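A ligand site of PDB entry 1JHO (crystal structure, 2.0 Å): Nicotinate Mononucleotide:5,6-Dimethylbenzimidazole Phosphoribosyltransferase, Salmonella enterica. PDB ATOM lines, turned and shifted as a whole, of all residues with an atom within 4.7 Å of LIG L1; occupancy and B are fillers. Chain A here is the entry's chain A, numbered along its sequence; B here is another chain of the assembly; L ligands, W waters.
OE2 of Glu 317 lies within hydrogen-bond range of N1 of LIG L1, at 2.6 Å. The side-chain carboxylate of Glu 174 lies within hydrogen-bond range of an oxygen (O7) of LIG L1, at 2.6 Å. An oxygen (O3) of LIG L1 lies within hydrogen-bond range of the backbone NH of Ala 178, at 2.7 Å. An oxygen (O2) of LIG L1 is in hydrogen-bond range of the backbone NH (N) of Ala 203, at 2.7 Å. O1 of LIG L1 is in hydrogen-bond range of N of Thr 180, 3.0 Å away. O1 of LIG L1 lies within hydrogen-bond range of OG1 of Thr 180 (2.8 Å). The side-chain sulfur (SD) of Met 177 lies close to an oxygen (O6) of LIG L1 (3.8 Å). The backbone NH (N) of Gly 176 lies within hydrogen-bond range of an oxygen (O6) of LIG L1, 3.0 Å away. O1 of LIG L1 is in hydrogen-bond range of N of Asn 179.
Water W1 bridges O2 of LIG L1 (2.7 Å) and O of Val 77 (2.8 Å). Water W2 lies within hydrogen-bond range of the side-chain hydroxyl of Thr 181 (2.7 Å), an oxygen (O1) of LIG L1 (2.8 Å), the backbone carbonyl oxygen of Val 77 (3.0 Å), the backbone carbonyl oxygen of Ala 178 (3.3 Å) and the side-chain hydroxyl of Thr 180 (3.5 Å). Water W3 lies within hydrogen-bond range of O2 of LIG L1 (2.8 Å) and O of Ala 203 (3.1 Å).
N2 of LIG L1 sits close to O of Leu 315 (3.2 Å). Merely in contact with LIG L1: Ala 78 (3.7 Å), Ser 80 (3.8 Å), Val 84 (3.7 Å), Gln 88 (3.7 Å), Leu 175 (3.6 Å), Gly 202 (3.6 Å) and Pro 32 of chain B (3.7 Å). 16 residues have an atom within 4 Å of LIG L1: Ala 78, Ser 80, Val 84, Gln 88, Glu 174, Leu 175, Gly 176, Met 177, Ala 178, Asn 179, Thr 180, Gly 202, Ala 203, Leu 315, Glu 317 and Pro 32 of chain B. The nearest printed residue that does not touch LIG L1 is Leu 348 of chain B (4.2 Å).
OE2 of Glu 174 sits at hydrogen-bond distance from N of Glu 317, 2.9 Å away. The side-chain amide nitrogen (NE2) of Gln 88 is in hydrogen-bond range of the side-chain carboxylate (OE2) of Glu 317, 3.0 Å away. The side-chain amide nitrogen (ND2) of Asn 179 is in hydrogen-bond range of the side-chain carboxylate (OE1) of Glu 174 (2.8 Å). The side-chain hydroxyl (OG) of Ser 80 lies close to the side-chain sulfur (SD) of Met 177, 3.8 Å away. The side-chain amide oxygen (OD1) of Asn 179 sits close to the backbone carbonyl oxygen (O) of Gly 176 (3.1 Å).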
ATOM      1  N   VAL A  77      -8.481 -10.834  31.513  1.00  0.00           N
ATOM      2  CA  VAL A  77      -8.885 -11.691  30.399  1.00  0.00           C
ATOM      3  C   VAL A  77      -8.029 -12.951  30.175  1.00  0.00           C
ATOM      4  O   VAL A  77      -8.366 -13.774  29.310  1.00  0.00           O
ATOM      5  CB  VAL A  77      -9.009 -10.908  29.085  1.00  0.00           C
ATOM      6  CG1 VAL A  77     -10.018  -9.765  29.230  1.00  0.00           C
ATOM      7  CG2 VAL A  77      -7.649 -10.380  28.636  1.00  0.00           C
ATOM      8  N   ALA A  78      -6.936 -13.082  30.940  1.00  0.00           N
ATOM      9  CA  ALA A  78      -5.999 -14.221  30.783  1.00  0.00           C
ATOM     10  C   ALA A  78      -5.522 -14.799  32.122  1.00  0.00           C
ATOM     11  O   ALA A  78      -5.121 -14.073  33.020  1.00  0.00           O
ATOM     12  CB  ALA A  78      -4.790 -13.795  29.966  1.00  0.00           C
ATOM     13  N   SER A  80      -2.912 -16.950  32.412  1.00  0.00           N
ATOM     14  CA  SER A  80      -1.469 -17.164  32.455  1.00  0.00           C
ATOM     15  C   SER A  80      -0.789 -15.916  32.987  1.00  0.00           C
ATOM     16  O   SER A  80      -1.103 -14.793  32.589  1.00  0.00           O
ATOM     17  CB  SER A  80      -0.836 -17.493  31.096  1.00  0.00           C
ATOM     18  OG  SER A  80      -1.539 -18.491  30.367  1.00  0.00           O
ATOM     19  N   VAL A  84       4.850 -15.233  31.613  1.00  0.00           N
ATOM     20  CA  VAL A  84       4.928 -16.435  30.803  1.00  0.00           C
ATOM     21  C   VAL A  84       5.405 -16.164  29.375  1.00  0.00           C
ATOM     22  O   VAL A  84       6.112 -16.979  28.772  1.00  0.00           O
ATOM     23  CB  VAL A  84       3.665 -17.301  30.878  1.00  0.00           C
ATOM     24  CG1 VAL A  84       3.773 -18.514  29.941  1.00  0.00           C
ATOM     25  CG2 VAL A  84       3.429 -17.752  32.329  1.00  0.00           C
ATOM     26  N   GLN A  88       8.432 -18.364  28.044  1.00  0.00           N
ATOM     27  CA  GLN A  88       8.191 -19.219  26.899  1.00  0.00           C
ATOM     28  C   GLN A  88       9.067 -18.788  25.710  1.00  0.00           C
ATOM     29  O   GLN A  88       9.546 -19.595  24.901  1.00  0.00           O
ATOM     30  CB  GLN A  88       6.712 -19.142  26.484  1.00  0.00           C
ATOM     31  CG  GLN A  88       5.811 -20.334  26.841  1.00  0.00           C
ATOM     32  CD  GLN A  88       6.336 -21.721  26.531  1.00  0.00           C
ATOM     33  OE1 GLN A  88       7.221 -22.236  27.230  1.00  0.00           O
ATOM     34  NE2 GLN A  88       5.735 -22.394  25.548  1.00  0.00           N
ATOM     35  N   GLU A 174       2.728 -17.160  17.108  1.00  0.00           N
ATOM     36  CA  GLU A 174       2.840 -16.093  18.099  1.00  0.00           C
ATOM     37  C   GLU A 174       2.976 -16.655  19.507  1.00  0.00           C
ATOM     38  O   GLU A 174       2.927 -17.856  19.774  1.00  0.00           O
ATOM     39  CB  GLU A 174       1.606 -15.167  18.039  1.00  0.00           C
ATOM     40  CG  GLU A 174       0.264 -15.943  17.890  1.00  0.00           C
ATOM     41  CD  GLU A 174       0.057 -16.963  18.995  1.00  0.00           C
ATOM     42  OE1 GLU A 174      -0.066 -16.681  20.166  1.00  0.00           O
ATOM     43  OE2 GLU A 174       0.055 -18.188  18.554  1.00  0.00           O
ATOM     44  N   LEU A 175       3.148 -15.704  20.401  1.00  0.00           N
ATOM     45  CA  LEU A 175       3.264 -15.931  21.830  1.00  0.00           C
ATOM     46  C   LEU A 175       2.896 -14.592  22.476  1.00  0.00           C
ATOM     47  O   LEU A 175       3.415 -13.548  22.080  1.00  0.00           O
ATOM     48  CB  LEU A 175       4.688 -16.392  22.183  1.00  0.00           C
ATOM     49  CG  LEU A 175       4.908 -17.069  23.524  1.00  0.00           C
ATOM     50  CD1 LEU A 175       4.141 -18.395  23.580  1.00  0.00           C
ATOM     51  CD2 LEU A 175       6.416 -17.302  23.671  1.00  0.00           C
ATOM     52  N   GLY A 176       1.956 -14.609  23.416  1.00  0.00           N
ATOM     53  CA  GLY A 176       1.534 -13.377  24.063  1.00  0.00           C
ATOM     54  C   GLY A 176       0.278 -13.594  24.898  1.00  0.00           C
ATOM     55  O   GLY A 176      -0.842 -13.672  24.364  1.00  0.00           O
ATOM     56  N   MET A 177       0.475 -13.691  26.214  1.00  0.00           N
ATOM     57  CA  MET A 177      -0.627 -13.883  27.133  1.00  0.00           C
ATOM     58  C   MET A 177      -1.665 -12.800  26.898  1.00  0.00           C
ATOM     59  O   MET A 177      -1.309 -11.601  26.771  1.00  0.00           O
ATOM     60  CB  MET A 177      -0.146 -13.852  28.601  1.00  0.00           C
ATOM     61  CG  MET A 177       1.068 -14.736  28.840  1.00  0.00           C
ATOM     62  SD  MET A 177       0.792 -16.433  28.267  1.00  0.00           S
ATOM     63  CE  MET A 177       2.088 -16.661  27.002  1.00  0.00           C
ATOM     64  N   ALA A 178      -2.934 -13.213  26.842  1.00  0.00           N
ATOM     65  CA  ALA A 178      -4.071 -12.306  26.621  1.00  0.00           C
ATOM     66  C   ALA A 178      -4.349 -12.005  25.134  1.00  0.00           C
ATOM     67  O   ALA A 178      -5.312 -11.303  24.799  1.00  0.00           O
ATOM     68  CB  ALA A 178      -3.954 -11.007  27.431  1.00  0.00           C
ATOM     69  N   ASN A 179      -3.513 -12.544  24.242  1.00  0.00           N
ATOM     70  CA  ASN A 179      -3.654 -12.289  22.812  1.00  0.00           C
ATOM     71  C   ASN A 179      -4.936 -12.749  22.131  1.00  0.00           C
ATOM     72  O   ASN A 179      -5.281 -12.265  21.042  1.00  0.00           O
ATOM     73  CB  ASN A 179      -2.374 -12.491  21.957  1.00  0.00           C
ATOM     74  CG  ASN A 179      -1.969 -13.927  21.687  1.00  0.00           C
ATOM     75  OD1 ASN A 179      -2.652 -14.877  22.095  1.00  0.00           O
ATOM     76  ND2 ASN A 179      -0.840 -14.067  20.988  1.00  0.00           N
ATOM     77  N   THR A 180      -5.672 -13.680  22.749  1.00  0.00           N
ATOM     78  CA  THR A 180      -6.914 -14.104  22.098  1.00  0.00           C
ATOM     79  C   THR A 180      -8.015 -13.042  22.203  1.00  0.00           C
ATOM     80  O   THR A 180      -9.055 -13.079  21.524  1.00  0.00           O
ATOM     81  CB  THR A 180      -7.391 -15.500  22.548  1.00  0.00           C
ATOM     82  OG1 THR A 180      -7.738 -15.472  23.920  1.00  0.00           O
ATOM     83  CG2 THR A 180      -6.277 -16.510  22.341  1.00  0.00           C
ATOM     84  N   THR A 181      -7.748 -12.070  23.078  1.00  0.00           N
ATOM     85  CA  THR A 181      -8.661 -10.975  23.268  1.00  0.00           C
ATOM     86  C   THR A 181      -8.644 -10.002  22.073  1.00  0.00           C
ATOM     87  O   THR A 181      -9.685  -9.769  21.450  1.00  0.00           O
ATOM     88  CB  THR A 181      -8.458 -10.278  24.629  1.00  0.00           C
ATOM     89  OG1 THR A 181      -8.786 -11.207  25.635  1.00  0.00           O
ATOM     90  CG2 THR A 181      -9.382  -9.063  24.740  1.00  0.00           C
ATOM     91  N   ILE A 201     -12.308 -19.383  25.096  1.00  0.00           N
ATOM     92  CA  ILE A 201     -11.610 -19.514  26.358  1.00  0.00           C
ATOM     93  C   ILE A 201     -10.109 -19.308  26.254  1.00  0.00           C
ATOM     94  O   ILE A 201      -9.420 -19.396  27.272  1.00  0.00           O
ATOM     95  CB  ILE A 201     -11.910 -20.803  27.110  1.00  0.00           C
ATOM     96  CG1 ILE A 201     -11.491 -21.966  26.225  1.00  0.00           C
ATOM     97  CG2 ILE A 201     -13.380 -20.897  27.447  1.00  0.00           C
ATOM     98  CD1 ILE A 201     -10.848 -23.114  26.983  1.00  0.00           C
ATOM     99  N   GLY A 202      -9.591 -19.068  25.058  1.00  0.00           N
ATOM    100  CA  GLY A 202      -8.149 -18.853  24.972  1.00  0.00           C
ATOM    101  C   GLY A 202      -7.399 -19.966  25.701  1.00  0.00           C
ATOM    102  O   GLY A 202      -7.698 -21.147  25.561  1.00  0.00           O
ATOM    103  N   ALA A 203      -6.420 -19.581  26.508  1.00  0.00           N
ATOM    104  CA  ALA A 203      -5.660 -20.589  27.198  1.00  0.00           C
ATOM    105  C   ALA A 203      -6.284 -20.988  28.530  1.00  0.00           C
ATOM    106  O   ALA A 203      -5.806 -20.639  29.605  1.00  0.00           O
ATOM    107  CB  ALA A 203      -4.193 -20.195  27.355  1.00  0.00           C
ATOM    108  N   LEU A 315      -3.140 -24.403  20.964  1.00  0.00           N
ATOM    109  CA  LEU A 315      -1.932 -23.998  21.633  1.00  0.00           C
ATOM    110  C   LEU A 315      -1.351 -22.701  21.068  1.00  0.00           C
ATOM    111  O   LEU A 315      -0.779 -21.891  21.802  1.00  0.00           O
ATOM    112  CB  LEU A 315      -0.861 -25.109  21.539  1.00  0.00           C
ATOM    113  CG  LEU A 315       0.557 -24.724  22.038  1.00  0.00           C
ATOM    114  CD1 LEU A 315       0.538 -24.293  23.502  1.00  0.00           C
ATOM    115  CD2 LEU A 315       1.478 -25.945  21.896  1.00  0.00           C
ATOM    116  N   GLY A 316      -1.434 -22.543  19.730  1.00  0.00           N
ATOM    117  CA  GLY A 316      -0.824 -21.415  19.069  1.00  0.00           C
ATOM    118  C   GLY A 316       0.673 -21.725  18.854  1.00  0.00           C
ATOM    119  O   GLY A 316       1.049 -22.919  18.742  1.00  0.00           O
ATOM    120  N   GLU A 317       1.499 -20.665  18.822  1.00  0.00           N
ATOM    121  CA  GLU A 317       2.959 -20.718  18.630  1.00  0.00           C
ATOM    122  C   GLU A 317       3.369 -21.103  17.193  1.00  0.00           C
ATOM    123  O   GLU A 317       4.545 -21.139  16.835  1.00  0.00           O
ATOM    124  CB  GLU A 317       3.660 -21.748  19.578  1.00  0.00           C
ATOM    125  CG  GLU A 317       3.228 -21.727  21.052  1.00  0.00           C
ATOM    126  CD  GLU A 317       4.058 -22.684  21.864  1.00  0.00           C
ATOM    127  OE1 GLU A 317       4.826 -23.486  21.358  1.00  0.00           O
ATOM    128  OE2 GLU A 317       3.887 -22.574  23.166  1.00  0.00           O
ATOM    129  N   LEU B  30       5.118 -28.237  28.815  1.00  0.00           N
ATOM    130  CA  LEU B  30       5.197 -26.783  28.643  1.00  0.00           C
ATOM    131  C   LEU B  30       4.048 -26.207  27.796  1.00  0.00           C
ATOM    132  O   LEU B  30       4.269 -25.704  26.681  1.00  0.00           O
ATOM    133  CB  LEU B  30       6.526 -26.503  27.933  1.00  0.00           C
ATOM    134  CG  LEU B  30       7.474 -25.465  28.522  1.00  0.00           C
ATOM    135  CD1 LEU B  30       7.222 -25.218  30.007  1.00  0.00           C
ATOM    136  CD2 LEU B  30       8.892 -25.944  28.278  1.00  0.00           C
ATOM    137  N   LYS B  31       2.827 -26.246  28.311  1.00  0.00           N
ATOM    138  CA  LYS B  31       1.680 -25.746  27.555  1.00  0.00           C
ATOM    139  C   LYS B  31       0.449 -25.763  28.433  1.00  0.00           C
ATOM    140  O   LYS B  31       0.430 -26.486  29.437  1.00  0.00           O
ATOM    141  CB  LYS B  31       1.347 -26.686  26.382  1.00  0.00           C
ATOM    142  CG  LYS B  31       1.031 -28.103  26.860  1.00  0.00           C
ATOM    143  CD  LYS B  31       0.494 -29.018  25.770  1.00  0.00           C
ATOM    144  CE  LYS B  31       0.458 -30.467  26.235  1.00  0.00           C
ATOM    145  NZ  LYS B  31      -0.426 -30.676  27.380  1.00  0.00           N
ATOM    146  N   PRO B  32      -0.593 -25.031  28.049  1.00  0.00           N
ATOM    147  CA  PRO B  32      -1.798 -25.092  28.843  1.00  0.00           C
ATOM    148  C   PRO B  32      -2.352 -26.516  28.739  1.00  0.00           C
ATOM    149  O   PRO B  32      -2.333 -27.139  27.679  1.00  0.00           O
ATOM    150  CB  PRO B  32      -2.787 -24.053  28.296  1.00  0.00           C
ATOM    151  CG  PRO B  32      -2.022 -23.268  27.230  1.00  0.00           C
ATOM    152  CD  PRO B  32      -0.705 -23.987  26.992  1.00  0.00           C
ATOM    153  N   LEU B 341       6.467 -27.713  32.522  1.00  0.00           N
ATOM    154  CA  LEU B 341       6.051 -26.509  33.185  1.00  0.00           C
ATOM    155  C   LEU B 341       6.887 -26.228  34.441  1.00  0.00           C
ATOM    156  O   LEU B 341       7.418 -25.140  34.649  1.00  0.00           O
ATOM    157  CB  LEU B 341       4.579 -26.637  33.601  1.00  0.00           C
ATOM    158  CG  LEU B 341       3.575 -26.444  32.455  1.00  0.00           C
ATOM    159  CD1 LEU B 341       2.159 -26.769  32.950  1.00  0.00           C
ATOM    160  CD2 LEU B 341       3.638 -24.999  31.952  1.00  0.00           C
ATOM    161  N   ILE B 346       6.866 -22.401  35.777  1.00  0.00           N
ATOM    162  CA  ILE B 346       5.576 -21.953  35.324  1.00  0.00           C
ATOM    163  C   ILE B 346       4.452 -22.634  36.072  1.00  0.00           C
ATOM    164  O   ILE B 346       4.350 -23.860  36.107  1.00  0.00           O
ATOM    165  CB  ILE B 346       5.367 -22.043  33.814  1.00  0.00           C
ATOM    166  CG1 ILE B 346       6.371 -21.161  33.090  1.00  0.00           C
ATOM    167  CG2 ILE B 346       3.953 -21.591  33.487  1.00  0.00           C
ATOM    168  CD1 ILE B 346       6.513 -21.540  31.608  1.00  0.00           C
ATOM    169  N   LEU B 348       0.335 -22.740  36.400  1.00  0.00           N
ATOM    170  CA  LEU B 348      -0.974 -22.403  35.874  1.00  0.00           C
ATOM    171  C   LEU B 348      -2.039 -22.955  36.794  1.00  0.00           C
ATOM    172  O   LEU B 348      -1.765 -23.799  37.659  1.00  0.00           O
ATOM    173  CB  LEU B 348      -1.158 -22.879  34.417  1.00  0.00           C
ATOM    174  CG  LEU B 348      -0.009 -22.455  33.485  1.00  0.00           C
ATOM    175  CD1 LEU B 348      -0.088 -23.203  32.152  1.00  0.00           C
ATOM    176  CD2 LEU B 348      -0.026 -20.946  33.240  1.00  0.00           C
HETATM  177  N1  LIG L   1       1.945 -21.176  24.117  1.00  0.00           N
HETATM  178  N2  LIG L   1       0.007 -20.010  24.241  1.00  0.00           N
HETATM  179  C1  LIG L   1       0.978 -20.532  23.453  1.00  0.00           C
HETATM  180  C2  LIG L   1       0.457 -20.311  25.543  1.00  0.00           C
HETATM  181  C3  LIG L   1       1.625 -21.056  25.454  1.00  0.00           C
HETATM  182  C4  LIG L   1       2.257 -21.558  26.592  1.00  0.00           C
HETATM  183  C5  LIG L   1       1.707 -21.287  27.840  1.00  0.00           C
HETATM  184  C6  LIG L   1       0.512 -20.526  27.948  1.00  0.00           C
HETATM  185  C7  LIG L   1      -0.109 -20.026  26.810  1.00  0.00           C
HETATM  186  C8  LIG L   1       2.388 -21.837  29.089  1.00  0.00           C
HETATM  187  P1  LIG L   1      -4.981 -16.176  26.284  1.00  0.00           P
HETATM  188  O1  LIG L   1      -5.449 -15.043  25.431  1.00  0.00           O
HETATM  189  O2  LIG L   1      -5.964 -16.939  27.111  1.00  0.00           O
HETATM  190  O3  LIG L   1      -3.740 -15.786  27.014  1.00  0.00           O
HETATM  191  O4  LIG L   1      -4.343 -17.210  25.224  1.00  0.00           O
HETATM  192  C9  LIG L   1      -3.328 -16.794  24.298  1.00  0.00           C
HETATM  193  C10 LIG L   1      -1.975 -17.252  24.792  1.00  0.00           C
HETATM  194  O5  LIG L   1      -1.936 -18.715  24.924  1.00  0.00           O
HETATM  195  C11 LIG L   1      -0.837 -16.932  23.862  1.00  0.00           C
HETATM  196  O6  LIG L   1       0.437 -16.944  24.524  1.00  0.00           O
HETATM  197  C12 LIG L   1      -0.993 -18.124  22.906  1.00  0.00           C
HETATM  198  O7  LIG L   1       0.262 -18.303  22.217  1.00  0.00           O
HETATM  199  C13 LIG L   1      -1.246 -19.308  23.845  1.00  0.00           C
HETATM  200  N1  LG2 L   2      -3.857 -19.839  21.999  1.00  0.00           N
HETATM  201  C1  LG2 L   2      -3.782 -20.097  20.659  1.00  0.00           C
HETATM  202  C2  LG2 L   2      -4.915 -20.585  20.012  1.00  0.00           C
HETATM  203  C3  LG2 L   2      -6.147 -20.789  20.718  1.00  0.00           C
HETATM  204  C4  LG2 L   2      -6.084 -20.471  22.078  1.00  0.00           C
HETATM  205  C5  LG2 L   2      -4.995 -20.011  22.785  1.00  0.00           C
HETATM  206  C6  LG2 L   2      -4.862 -20.896  18.520  1.00  0.00           C
HETATM  207  O1  LG2 L   2      -5.897 -21.334  17.942  1.00  0.00           O
HETATM  208  O2  LG2 L   2      -3.785 -20.711  17.856  1.00  0.00           O
HETATM  209  O   HOH W   1      -8.469 -16.005  27.572  1.00  0.00           O
HETATM  210  O   HOH W   2      -7.261 -13.279  26.555  1.00  0.00           O
HETATM  211  O   HOH W   3      -6.146 -17.516  29.829  1.00  0.00           O
